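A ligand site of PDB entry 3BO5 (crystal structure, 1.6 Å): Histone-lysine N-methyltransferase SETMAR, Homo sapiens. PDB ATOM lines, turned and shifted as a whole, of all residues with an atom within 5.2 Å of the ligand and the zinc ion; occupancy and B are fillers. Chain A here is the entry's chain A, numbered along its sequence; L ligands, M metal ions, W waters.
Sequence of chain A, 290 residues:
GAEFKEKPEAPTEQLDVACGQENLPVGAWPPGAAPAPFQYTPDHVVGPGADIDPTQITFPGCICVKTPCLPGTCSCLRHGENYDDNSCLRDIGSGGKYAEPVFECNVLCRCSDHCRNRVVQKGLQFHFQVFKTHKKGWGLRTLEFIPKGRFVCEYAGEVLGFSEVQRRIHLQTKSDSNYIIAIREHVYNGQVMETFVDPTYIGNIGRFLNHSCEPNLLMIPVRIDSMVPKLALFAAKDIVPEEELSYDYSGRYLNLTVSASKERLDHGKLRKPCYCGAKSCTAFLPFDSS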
ATOM      1  N   LYS A 135     -23.953 -34.537  27.939  1.00  0.00           N
ATOM      2  CA  LYS A 135     -25.251 -33.892  28.278  1.00  0.00           C
ATOM      3  C   LYS A 135     -26.124 -33.444  27.119  1.00  0.00           C
ATOM      4  O   LYS A 135     -27.164 -32.844  27.345  1.00  0.00           O
ATOM      5  CB  LYS A 135     -24.943 -32.660  29.099  1.00  0.00           C
ATOM      6  CG  LYS A 135     -24.449 -33.013  30.486  1.00  0.00           C
ATOM      7  CD  LYS A 135     -24.151 -31.818  31.272  1.00  0.00           C
ATOM      8  CE  LYS A 135     -25.482 -31.213  31.679  1.00  0.00           C
ATOM      9  NZ  LYS A 135     -25.296 -30.135  32.567  1.00  0.00           N
ATOM     10  N   LYS A 136     -25.666 -33.652  25.881  1.00  0.00           N
ATOM     11  CA  LYS A 136     -26.327 -33.093  24.689  1.00  0.00           C
ATOM     12  C   LYS A 136     -26.908 -34.198  23.808  1.00  0.00           C
ATOM     13  O   LYS A 136     -27.348 -33.930  22.680  1.00  0.00           O
ATOM     14  CB  LYS A 136     -25.285 -32.260  23.904  1.00  0.00           C
ATOM     15  CG  LYS A 136     -24.669 -31.110  24.726  1.00  0.00           C
ATOM     16  CD  LYS A 136     -23.570 -30.390  23.927  1.00  0.00           C
ATOM     17  CE  LYS A 136     -22.506 -31.313  23.414  1.00  0.00           C
ATOM     18  NZ  LYS A 136     -21.293 -30.429  23.036  1.00  0.00           N
ATOM     19  N   GLY A 137     -27.002 -35.453  24.318  1.00  0.00           N
ATOM     20  CA  GLY A 137     -27.464 -36.573  23.492  1.00  0.00           C
ATOM     21  C   GLY A 137     -26.394 -36.966  22.554  1.00  0.00           C
ATOM     22  O   GLY A 137     -25.212 -36.915  22.901  1.00  0.00           O
ATOM     23  N   TRP A 138     -26.774 -37.421  21.357  1.00  0.00           N
ATOM     24  CA  TRP A 138     -25.749 -37.864  20.425  1.00  0.00           C
ATOM     25  C   TRP A 138     -25.134 -36.644  19.763  1.00  0.00           C
ATOM     26  O   TRP A 138     -25.774 -35.563  19.685  1.00  0.00           O
ATOM     27  CB  TRP A 138     -26.360 -38.737  19.324  1.00  0.00           C
ATOM     28  CG  TRP A 138     -26.798 -40.026  19.900  1.00  0.00           C
ATOM     29  CD1 TRP A 138     -28.006 -40.304  20.502  1.00  0.00           C
ATOM     30  CD2 TRP A 138     -25.980 -41.175  20.058  1.00  0.00           C
ATOM     31  NE1 TRP A 138     -27.991 -41.635  20.963  1.00  0.00           N
ATOM     32  CE2 TRP A 138     -26.761 -42.156  20.717  1.00  0.00           C
ATOM     33  CE3 TRP A 138     -24.678 -41.478  19.688  1.00  0.00           C
ATOM     34  CZ2 TRP A 138     -26.279 -43.449  20.976  1.00  0.00           C
ATOM     35  CZ3 TRP A 138     -24.208 -42.795  19.906  1.00  0.00           C
ATOM     36  CH2 TRP A 138     -24.996 -43.728  20.600  1.00  0.00           C
ATOM     37  N   GLY A 139     -23.871 -36.742  19.372  1.00  0.00           N
ATOM     38  CA  GLY A 139     -23.232 -35.684  18.568  1.00  0.00           C
ATOM     39  C   GLY A 139     -22.446 -36.306  17.432  1.00  0.00           C
ATOM     40  O   GLY A 139     -22.423 -37.539  17.285  1.00  0.00           O
ATOM     41  N   ASP A 176     -38.029 -33.938  22.862  1.00  0.00           N
ATOM     42  CA  ASP A 176     -37.739 -34.079  21.422  1.00  0.00           C
ATOM     43  C   ASP A 176     -36.449 -33.314  21.040  1.00  0.00           C
ATOM     44  O   ASP A 176     -36.283 -32.144  21.451  1.00  0.00           O
ATOM     45  CB  ASP A 176     -38.900 -33.558  20.549  1.00  0.00           C
ATOM     46  CG  ASP A 176     -40.137 -34.466  20.579  1.00  0.00           C
ATOM     47  OD1 ASP A 176     -40.049 -35.591  21.125  1.00  0.00           O
ATOM     48  OD2 ASP A 176     -41.186 -34.061  20.036  1.00  0.00           O
ATOM     49  N   SER A 177     -35.559 -33.967  20.295  1.00  0.00           N
ATOM     50  CA  SER A 177     -34.470 -33.229  19.620  1.00  0.00           C
ATOM     51  C   SER A 177     -35.199 -32.477  18.494  1.00  0.00           C
ATOM     52  O   SER A 177     -36.182 -32.997  17.913  1.00  0.00           O
ATOM     53  CB  SER A 177     -33.400 -34.182  19.075  1.00  0.00           C
ATOM     54  OG  SER A 177     -32.763 -34.917  20.136  1.00  0.00           O
ATOM     55  N   ASN A 178     -34.802 -31.228  18.240  1.00  0.00           N
ATOM     56  CA  ASN A 178     -35.474 -30.339  17.244  1.00  0.00           C
ATOM     57  C   ASN A 178     -34.495 -30.235  16.085  1.00  0.00           C
ATOM     58  O   ASN A 178     -33.321 -29.899  16.355  1.00  0.00           O
ATOM     59  CB  ASN A 178     -35.608 -28.963  17.856  1.00  0.00           C
ATOM     60  CG  ASN A 178     -36.501 -28.969  19.088  1.00  0.00           C
ATOM     61  OD1 ASN A 178     -36.014 -28.931  20.253  1.00  0.00           O
ATOM     62  ND2 ASN A 178     -37.770 -29.081  18.862  1.00  0.00           N
ATOM     63  N   TYR A 179     -34.933 -30.529  14.849  1.00  0.00           N
ATOM     64  CA  TYR A 179     -33.961 -30.518  13.733  1.00  0.00           C
ATOM     65  C   TYR A 179     -34.280 -29.612  12.571  1.00  0.00           C
ATOM     66  O   TYR A 179     -33.453 -29.449  11.675  1.00  0.00           O
ATOM     67  CB  TYR A 179     -33.844 -31.954  13.125  1.00  0.00           C
ATOM     68  CG  TYR A 179     -33.415 -33.068  14.038  1.00  0.00           C
ATOM     69  CD1 TYR A 179     -34.358 -33.802  14.724  1.00  0.00           C
ATOM     70  CD2 TYR A 179     -32.083 -33.370  14.196  1.00  0.00           C
ATOM     71  CE1 TYR A 179     -33.952 -34.812  15.597  1.00  0.00           C
ATOM     72  CE2 TYR A 179     -31.649 -34.365  15.003  1.00  0.00           C
ATOM     73  CZ  TYR A 179     -32.593 -35.115  15.724  1.00  0.00           C
ATOM     74  OH  TYR A 179     -32.255 -36.116  16.600  1.00  0.00           O
ATOM     75  N   ARG A 207     -27.590 -34.125  10.792  1.00  0.00           N
ATOM     76  CA  ARG A 207     -28.630 -34.049  11.843  1.00  0.00           C
ATOM     77  C   ARG A 207     -28.009 -34.233  13.225  1.00  0.00           C
ATOM     78  O   ARG A 207     -28.616 -33.829  14.218  1.00  0.00           O
ATOM     79  CB  ARG A 207     -29.764 -35.066  11.629  1.00  0.00           C
ATOM     80  CG  ARG A 207     -29.255 -36.498  11.889  1.00  0.00           C
ATOM     81  CD  ARG A 207     -30.158 -37.490  11.292  1.00  0.00           C
ATOM     82  NE  ARG A 207     -31.514 -37.456  11.868  1.00  0.00           N
ATOM     83  CZ  ARG A 207     -31.840 -38.043  13.032  1.00  0.00           C
ATOM     84  NH1 ARG A 207     -30.875 -38.637  13.780  1.00  0.00           N
ATOM     85  NH2 ARG A 207     -33.139 -38.083  13.478  1.00  0.00           N
ATOM     86  N   PHE A 208     -26.819 -34.879  13.303  1.00  0.00           N
ATOM     87  CA  PHE A 208     -26.226 -35.093  14.639  1.00  0.00           C
ATOM     88  C   PHE A 208     -25.375 -33.971  15.166  1.00  0.00           C
ATOM     89  O   PHE A 208     -24.881 -34.037  16.281  1.00  0.00           O
ATOM     90  CB  PHE A 208     -25.387 -36.375  14.616  1.00  0.00           C
ATOM     91  CG  PHE A 208     -26.253 -37.612  14.506  1.00  0.00           C
ATOM     92  CD1 PHE A 208     -27.028 -38.012  15.617  1.00  0.00           C
ATOM     93  CD2 PHE A 208     -26.305 -38.367  13.332  1.00  0.00           C
ATOM     94  CE1 PHE A 208     -27.872 -39.143  15.512  1.00  0.00           C
ATOM     95  CE2 PHE A 208     -27.150 -39.481  13.229  1.00  0.00           C
ATOM     96  CZ  PHE A 208     -27.898 -39.893  14.351  1.00  0.00           C
ATOM     97  N   LEU A 209     -25.225 -32.899  14.385  1.00  0.00           N
ATOM     98  CA  LEU A 209     -24.414 -31.775  14.839  1.00  0.00           C
ATOM     99  C   LEU A 209     -25.053 -31.010  15.957  1.00  0.00           C
ATOM    100  O   LEU A 209     -26.166 -30.457  15.779  1.00  0.00           O
ATOM    101  CB  LEU A 209     -24.205 -30.818  13.713  1.00  0.00           C
ATOM    102  CG  LEU A 209     -23.323 -31.422  12.596  1.00  0.00           C
ATOM    103  CD1 LEU A 209     -23.489 -30.573  11.301  1.00  0.00           C
ATOM    104  CD2 LEU A 209     -21.838 -31.608  13.022  1.00  0.00           C
ATOM    105  N   ASN A 210     -24.339 -30.964  17.083  1.00  0.00           N
ATOM    106  CA  ASN A 210     -24.838 -30.120  18.172  1.00  0.00           C
ATOM    107  C   ASN A 210     -24.529 -28.636  17.978  1.00  0.00           C
ATOM    108  O   ASN A 210     -23.706 -28.241  17.128  1.00  0.00           O
ATOM    109  CB  ASN A 210     -24.311 -30.681  19.513  1.00  0.00           C
ATOM    110  CG  ASN A 210     -25.000 -31.956  19.872  1.00  0.00           C
ATOM    111  OD1 ASN A 210     -26.217 -32.070  19.727  1.00  0.00           O
ATOM    112  ND2 ASN A 210     -24.239 -32.933  20.378  1.00  0.00           N
ATOM    113  N   HIS A 211     -25.229 -27.788  18.756  1.00  0.00           N
ATOM    114  CA  HIS A 211     -24.962 -26.383  18.703  1.00  0.00           C
ATOM    115  C   HIS A 211     -23.765 -26.030  19.588  1.00  0.00           C
ATOM    116  O   HIS A 211     -23.537 -26.585  20.624  1.00  0.00           O
ATOM    117  CB  HIS A 211     -26.150 -25.691  19.422  1.00  0.00           C
ATOM    118  CG  HIS A 211     -25.907 -24.263  19.709  1.00  0.00           C
ATOM    119  ND1 HIS A 211     -25.908 -23.297  18.714  1.00  0.00           N
ATOM    120  CD2 HIS A 211     -25.607 -23.626  20.874  1.00  0.00           C
ATOM    121  CE1 HIS A 211     -25.617 -22.123  19.264  1.00  0.00           C
ATOM    122  NE2 HIS A 211     -25.401 -22.306  20.567  1.00  0.00           N
ATOM    123  N   SER A 212     -23.031 -25.036  19.162  1.00  0.00           N
ATOM    124  CA  SER A 212     -22.099 -24.413  20.046  1.00  0.00           C
ATOM    125  C   SER A 212     -22.179 -22.925  19.885  1.00  0.00           C
ATOM    126  O   SER A 212     -22.356 -22.464  18.780  1.00  0.00           O
ATOM    127  CB  SER A 212     -20.702 -24.877  19.693  1.00  0.00           C
ATOM    128  OG  SER A 212     -19.776 -24.123  20.550  1.00  0.00           O
ATOM    129  N   CYS A 213     -21.972 -22.181  21.005  1.00  0.00           N
ATOM    130  CA  CYS A 213     -21.899 -20.742  20.945  1.00  0.00           C
ATOM    131  C   CYS A 213     -20.595 -20.274  20.299  1.00  0.00           C
ATOM    132  O   CYS A 213     -20.463 -19.107  19.935  1.00  0.00           O
ATOM    133  CB  CYS A 213     -22.009 -20.261  22.421  1.00  0.00           C
ATOM    134  SG  CYS A 213     -23.685 -20.534  23.020  1.00  0.00           S
ATOM    135  N   TYR A 249     -26.670 -22.744  16.053  1.00  0.00           N
ATOM    136  CA  TYR A 249     -28.060 -22.930  15.657  1.00  0.00           C
ATOM    137  C   TYR A 249     -28.772 -21.591  15.334  1.00  0.00           C
ATOM    138  O   TYR A 249     -29.829 -21.635  14.705  1.00  0.00           O
ATOM    139  CB  TYR A 249     -28.850 -23.638  16.759  1.00  0.00           C
ATOM    140  CG  TYR A 249     -28.603 -25.117  16.863  1.00  0.00           C
ATOM    141  CD1 TYR A 249     -27.563 -25.742  16.163  1.00  0.00           C
ATOM    142  CD2 TYR A 249     -29.437 -25.910  17.670  1.00  0.00           C
ATOM    143  CE1 TYR A 249     -27.338 -27.123  16.314  1.00  0.00           C
ATOM    144  CE2 TYR A 249     -29.256 -27.271  17.786  1.00  0.00           C
ATOM    145  CZ  TYR A 249     -28.178 -27.872  17.096  1.00  0.00           C
ATOM    146  OH  TYR A 249     -28.032 -29.206  17.268  1.00  0.00           O
ATOM    147  N   ARG A 264     -32.241 -22.548  13.380  1.00  0.00           N
ATOM    148  CA  ARG A 264     -32.902 -23.773  13.809  1.00  0.00           C
ATOM    149  C   ARG A 264     -34.193 -23.461  14.551  1.00  0.00           C
ATOM    150  O   ARG A 264     -34.273 -22.505  15.316  1.00  0.00           O
ATOM    151  CB  ARG A 264     -31.987 -24.599  14.718  1.00  0.00           C
ATOM    152  CG  ARG A 264     -30.885 -25.214  13.921  1.00  0.00           C
ATOM    153  CD  ARG A 264     -31.298 -26.556  13.326  1.00  0.00           C
ATOM    154  NE  ARG A 264     -31.499 -27.649  14.254  1.00  0.00           N
ATOM    155  CZ  ARG A 264     -30.563 -28.573  14.544  1.00  0.00           C
ATOM    156  NH1 ARG A 264     -29.392 -28.533  13.888  1.00  0.00           N
ATOM    157  NH2 ARG A 264     -30.820 -29.543  15.406  1.00  0.00           N
ATOM    158  N   LYS A 272     -34.181 -23.486  26.099  1.00  0.00           N
ATOM    159  CA  LYS A 272     -33.497 -24.719  26.453  1.00  0.00           C
ATOM    160  C   LYS A 272     -32.067 -24.374  26.806  1.00  0.00           C
ATOM    161  O   LYS A 272     -31.494 -23.478  26.200  1.00  0.00           O
ATOM    162  CB  LYS A 272     -33.491 -25.643  25.252  1.00  0.00           C
ATOM    163  CG  LYS A 272     -34.912 -26.115  24.933  1.00  0.00           C
ATOM    164  CD  LYS A 272     -34.782 -27.376  24.149  1.00  0.00           C
ATOM    165  CE  LYS A 272     -36.138 -27.958  23.753  1.00  0.00           C
ATOM    166  NZ  LYS A 272     -35.852 -29.357  23.311  1.00  0.00           N
ATOM    167  N   PRO A 273     -31.520 -25.014  27.829  1.00  0.00           N
ATOM    168  CA  PRO A 273     -30.144 -24.664  28.267  1.00  0.00           C
ATOM    169  C   PRO A 273     -29.147 -25.174  27.264  1.00  0.00           C
ATOM    170  O   PRO A 273     -29.377 -26.227  26.662  1.00  0.00           O
ATOM    171  CB  PRO A 273     -29.933 -25.449  29.536  1.00  0.00           C
ATOM    172  CG  PRO A 273     -31.239 -26.011  29.878  1.00  0.00           C
ATOM    173  CD  PRO A 273     -32.136 -26.029  28.708  1.00  0.00           C
ATOM    174  N   CYS A 274     -28.068 -24.421  27.133  1.00  0.00           N
ATOM    175  CA  CYS A 274     -26.945 -24.799  26.265  1.00  0.00           C
ATOM    176  C   CYS A 274     -25.847 -25.318  27.192  1.00  0.00           C
ATOM    177  O   CYS A 274     -25.464 -24.670  28.170  1.00  0.00           O
ATOM    178  CB  CYS A 274     -26.419 -23.549  25.482  1.00  0.00           C
ATOM    179  SG  CYS A 274     -25.102 -24.077  24.403  1.00  0.00           S
ATOM    180  N   TYR A 275     -25.227 -26.420  26.763  1.00  0.00           N
ATOM    181  CA  TYR A 275     -24.119 -27.056  27.480  1.00  0.00           C
ATOM    182  C   TYR A 275     -22.867 -27.090  26.566  1.00  0.00           C
ATOM    183  O   TYR A 275     -22.035 -28.028  26.670  1.00  0.00           O
ATOM    184  CB  TYR A 275     -24.472 -28.483  27.942  1.00  0.00           C
ATOM    185  CG  TYR A 275     -25.755 -28.566  28.717  1.00  0.00           C
ATOM    186  CD1 TYR A 275     -25.921 -27.713  29.830  1.00  0.00           C
ATOM    187  CD2 TYR A 275     -26.725 -29.481  28.395  1.00  0.00           C
ATOM    188  CE1 TYR A 275     -27.092 -27.791  30.604  1.00  0.00           C
ATOM    189  CE2 TYR A 275     -27.926 -29.552  29.150  1.00  0.00           C
ATOM    190  CZ  TYR A 275     -28.066 -28.696  30.253  1.00  0.00           C
ATOM    191  OH  TYR A 275     -29.205 -28.760  31.057  1.00  0.00           O
ATOM    192  N   CYS A 276     -22.752 -26.120  25.664  1.00  0.00           N
ATOM    193  CA  CYS A 276     -21.690 -26.192  24.676  1.00  0.00           C
ATOM    194  C   CYS A 276     -20.341 -26.035  25.329  1.00  0.00           C
ATOM    195  O   CYS A 276     -19.387 -26.504  24.744  1.00  0.00           O
ATOM    196  CB  CYS A 276     -21.893 -25.164  23.552  1.00  0.00           C
ATOM    197  SG  CYS A 276     -21.445 -23.454  23.972  1.00  0.00           S
ATOM    198  N   GLY A 277     -20.255 -25.391  26.508  1.00  0.00           N
ATOM    199  CA  GLY A 277     -18.897 -25.268  27.201  1.00  0.00           C
ATOM    200  C   GLY A 277     -18.026 -24.148  26.745  1.00  0.00           C
ATOM    201  O   GLY A 277     -16.905 -23.934  27.256  1.00  0.00           O
ATOM    202  N   ALA A 278     -18.486 -23.393  25.761  1.00  0.00           N
ATOM    203  CA  ALA A 278     -17.708 -22.250  25.284  1.00  0.00           C
ATOM    204  C   ALA A 278     -17.632 -21.121  26.318  1.00  0.00           C
ATOM    205  O   ALA A 278     -18.610 -20.866  27.058  1.00  0.00           O
ATOM    206  CB  ALA A 278     -18.299 -21.732  23.939  1.00  0.00           C
ATOM    207  N   CYS A 281     -20.425 -18.805  26.074  1.00  0.00           N
ATOM    208  CA  CYS A 281     -21.788 -19.434  26.114  1.00  0.00           C
ATOM    209  C   CYS A 281     -22.856 -18.482  26.623  1.00  0.00           C
ATOM    210  O   CYS A 281     -22.619 -17.729  27.597  1.00  0.00           O
ATOM    211  CB  CYS A 281     -21.809 -20.707  26.910  1.00  0.00           C
ATOM    212  SG  CYS A 281     -23.375 -21.677  26.743  1.00  0.00           S
ATOM    213  N   THR A 282     -24.019 -18.456  25.963  1.00  0.00           N
ATOM    214  CA  THR A 282     -25.104 -17.575  26.387  1.00  0.00           C
ATOM    215  C   THR A 282     -26.006 -18.302  27.379  1.00  0.00           C
ATOM    216  O   THR A 282     -26.953 -17.683  27.936  1.00  0.00           O
ATOM    217  CB  THR A 282     -25.964 -17.256  25.192  1.00  0.00           C
ATOM    218  OG1 THR A 282     -26.493 -18.490  24.678  1.00  0.00           O
ATOM    219  CG2 THR A 282     -25.150 -16.559  24.136  1.00  0.00           C
ATOM    220  N   ALA A 283     -25.748 -19.609  27.597  1.00  0.00           N
ATOM    221  CA  ALA A 283     -26.503 -20.527  28.451  1.00  0.00           C
ATOM    222  C   ALA A 283     -27.837 -20.976  27.853  1.00  0.00           C
ATOM    223  O   ALA A 283     -28.547 -21.786  28.476  1.00  0.00           O
ATOM    224  CB  ALA A 283     -26.744 -19.903  29.909  1.00  0.00           C
ATOM    225  N   LEU A 285     -29.895 -22.452  24.214  1.00  0.00           N
ATOM    226  CA  LEU A 285     -29.842 -22.930  22.873  1.00  0.00           C
ATOM    227  C   LEU A 285     -30.712 -22.011  22.028  1.00  0.00           C
ATOM    228  O   LEU A 285     -31.939 -21.895  22.290  1.00  0.00           O
ATOM    229  CB  LEU A 285     -30.337 -24.405  22.905  1.00  0.00           C
ATOM    230  CG  LEU A 285     -29.682 -25.570  22.263  1.00  0.00           C
ATOM    231  CD1 LEU A 285     -28.184 -25.499  22.597  1.00  0.00           C
ATOM    232  CD2 LEU A 285     -30.397 -26.771  22.801  1.00  0.00           C
ATOM    233  N   PHE A 287     -32.735 -21.511  19.535  1.00  0.00           N
ATOM    234  CA  PHE A 287     -33.806 -21.817  18.548  1.00  0.00           C
ATOM    235  C   PHE A 287     -34.707 -20.617  18.339  1.00  0.00           C
ATOM    236  O   PHE A 287     -34.874 -19.789  19.251  1.00  0.00           O
ATOM    237  CB  PHE A 287     -34.659 -22.974  19.068  1.00  0.00           C
ATOM    238  CG  PHE A 287     -33.972 -24.280  19.093  1.00  0.00           C
ATOM    239  CD1 PHE A 287     -33.729 -24.993  17.913  1.00  0.00           C
ATOM    240  CD2 PHE A 287     -33.636 -24.868  20.318  1.00  0.00           C
ATOM    241  CE1 PHE A 287     -33.100 -26.275  17.954  1.00  0.00           C
ATOM    242  CE2 PHE A 287     -33.033 -26.095  20.383  1.00  0.00           C
ATOM    243  CZ  PHE A 287     -32.760 -26.835  19.197  1.00  0.00           C
HETATM  244  N1  LIG L   1     -28.180 -34.294  20.233  1.00  0.00           N
HETATM  245  C1  LIG L   1     -29.037 -34.594  19.046  1.00  0.00           C
HETATM  246  C2  LIG L   1     -28.390 -34.141  17.716  1.00  0.00           C
HETATM  247  C3  LIG L   1     -28.605 -32.622  17.543  1.00  0.00           C
HETATM  248  S1  LIG L   1     -30.352 -32.215  17.261  1.00  0.00           S
HETATM  249  C4  LIG L   1     -29.351 -36.110  19.045  1.00  0.00           C
HETATM  250  O1  LIG L   1     -29.067 -36.805  20.013  1.00  0.00           O
HETATM  251  O2  LIG L   1     -29.916 -36.587  18.001  1.00  0.00           O
HETATM  252  C5  LIG L   1     -30.550 -30.879  18.464  1.00  0.00           C
HETATM  253  C6  LIG L   1     -30.748 -31.353  19.907  1.00  0.00           C
HETATM  254  O3  LIG L   1     -29.504 -31.751  20.492  1.00  0.00           O
HETATM  255  C7  LIG L   1     -31.247 -30.264  20.819  1.00  0.00           C
HETATM  256  O4  LIG L   1     -32.697 -30.159  20.750  1.00  0.00           O
HETATM  257  C8  LIG L   1     -30.780 -30.695  22.176  1.00  0.00           C
HETATM  258  O5  LIG L   1     -31.502 -31.843  22.662  1.00  0.00           O
HETATM  259  C9  LIG L   1     -29.395 -31.232  21.832  1.00  0.00           C
HETATM  260  N2  LIG L   1     -28.365 -30.183  21.785  1.00  0.00           N
HETATM  261  C10 LIG L   1     -27.629 -29.751  20.678  1.00  0.00           C
HETATM  262  N3  LIG L   1     -26.751 -28.855  21.076  1.00  0.00           N
HETATM  263  C11 LIG L   1     -26.849 -28.712  22.420  1.00  0.00           C
HETATM  264  C12 LIG L   1     -26.162 -27.860  23.307  1.00  0.00           C
HETATM  265  N4  LIG L   1     -25.143 -27.057  22.999  1.00  0.00           N
HETATM  266  N5  LIG L   1     -26.580 -27.941  24.627  1.00  0.00           N
HETATM  267  C13 LIG L   1     -27.589 -28.773  25.020  1.00  0.00           C
HETATM  268  N6  LIG L   1     -28.269 -29.644  24.190  1.00  0.00           N
HETATM  269  C14 LIG L   1     -27.888 -29.507  22.885  1.00  0.00           C
HETATM  270 ZN    ZN M   1     -23.399 -22.406  24.555  1.00  0.00          ZN
HETATM  271  O   HOH W   1     -29.638 -31.237  25.906  1.00  0.00           O
HETATM  272  O   HOH W   2     -30.731 -38.028  21.750  1.00  0.00           O
HETATM  273  O   HOH W   3     -30.539 -39.205  18.096  1.00  0.00           O
HETATM  274  O   HOH W   4     -32.742 -29.706  24.728  1.00  0.00           O
HETATM  275  O   HOH W   5     -30.567 -34.426  21.937  1.00  0.00           O
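The zinc ion is bound by the side-chain sulfur (SG) of Cys 276 (2.3 Å), the side-chain sulfur (SG) of Cys 281 (2.3 Å), the side-chain sulfur (SG) of Cys 274 (2.4 Å) and the side-chain sulfur (SG) of Cys 213 (2.4 Å). The zinc ion has four donor atoms within binding distance.
Water W1 bridges N6 of the ligand (2.7 Å) and O of Lys 135 (3.3 Å). Water W5 lies within hydrogen-bond range of an oxygen (O5) of the ligand (2.8 Å), the side-chain hydroxyl of Ser 177 (2.9 Å) and the backbone carbonyl oxygen of Lys 136 (3.3 Å). Water W4 bridges an oxygen (O5) of the ligand and the side-chain amino group (NZ) of Lys 272.
Gly 137 touches the ligand. Ser 177 touches the ligand (CA to O4, 3.7 Å). O of Arg 207 touches C2 of the ligand (3.5 Å). Phe 208 touches the ligand. Leu 209 touches the ligand (O to C3, 3.7 Å). Pro 273 touches the ligand (O to C13, 3.5 Å). Leu 285 touches the ligand (CD1 to C12, 3.2 Å). CZ of Phe 287 touches O4 of the ligand, at 3.7 Å. Hydrophobic or aromatic side chains that line the ligand: Trp 138, Tyr 179, His 211, Tyr 249, Tyr 275, Leu 285 and Phe 287. Within 4 Å of the ligand: Lys 136, Gly 137, Trp 138, Ser 177, Asn 178, Tyr 179, Arg 207, Phe 208, Leu 209, Asn 210, His 211, Tyr 249, Arg 264, Pro 273, Cys 274, Tyr 275, Cys 276, Leu 285 and Phe 287. The nearest printed residue that does not touch the ligand is Lys 272 (4.1 Å).
Within 4 Å of the zinc ion: Cys 213, Cys 274, Cys 276 and Cys 281.
The backbone carbonyl oxygen of Asn 178 is in hydrogen-bond range of the guanidinium group of Arg 264 (2.7 Å). The backbone NH (N) of Tyr 249 is in hydrogen-bond range of a ring nitrogen (ND1) of His 211. SG of Cys 213 sits close to N of Thr 282 (3.6 Å). The side-chain amide oxygen (OD1) of Asn 178 sits at hydrogen-bond distance from the side-chain amino group (NZ) of Lys 272, at 3.1 Å. The backbone NH (N) of Cys 213 is in hydrogen-bond range of a ring nitrogen (NE2) of His 211 (3.5 Å). The side-chain sulfur of Cys 276 sits close to the backbone NH of Ala 278 (3.5 Å). The backbone carbonyl oxygen (O) of Lys 272 lies within hydrogen-bond range of the backbone NH (N) of Leu 285 (2.7 Å). The backbone carbonyl oxygen (O) of Ala 283 is in hydrogen-bond range of the backbone NH (N) of Cys 274 (3.0 Å).
OH of Tyr 249 sits close to S1 of the ligand (3.8 Å). The backbone carbonyl oxygen of Trp 138 sits at hydrogen-bond distance from a nitrogen (N1) of the ligand (2.8 Å). O1 of the ligand is in hydrogen-bond range of N of Trp 138 (2.7 Å). The side-chain amide oxygen (OD1) of Asn 210 sits close to a nitrogen (N1) of the ligand (3.0 Å). The side-chain sulfur (SG) of Cys 274 lies close to a nitrogen (N4) of the ligand (3.3 Å). The backbone NH (N) of Tyr 275 lies within hydrogen-bond range of a nitrogen (N5) of the ligand, 3.0 Å away. A nitrogen (N1) of the ligand is in hydrogen-bond range of the backbone carbonyl oxygen (O) of Lys 136, 2.6 Å away. N of Asn 178 is in hydrogen-bond range of O4 of the ligand (3.4 Å). The backbone carbonyl oxygen of His 211 sits at hydrogen-bond distance from a nitrogen (N4) of the ligand (2.9 Å). N3 of the ligand is in hydrogen-bond range of N of His 211 (3.0 Å). S1 of the ligand lies close to NH2 of Arg 264, at 3.3 Å. OH of Tyr 179 lies within hydrogen-bond range of O2 of the ligand (2.8 Å).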
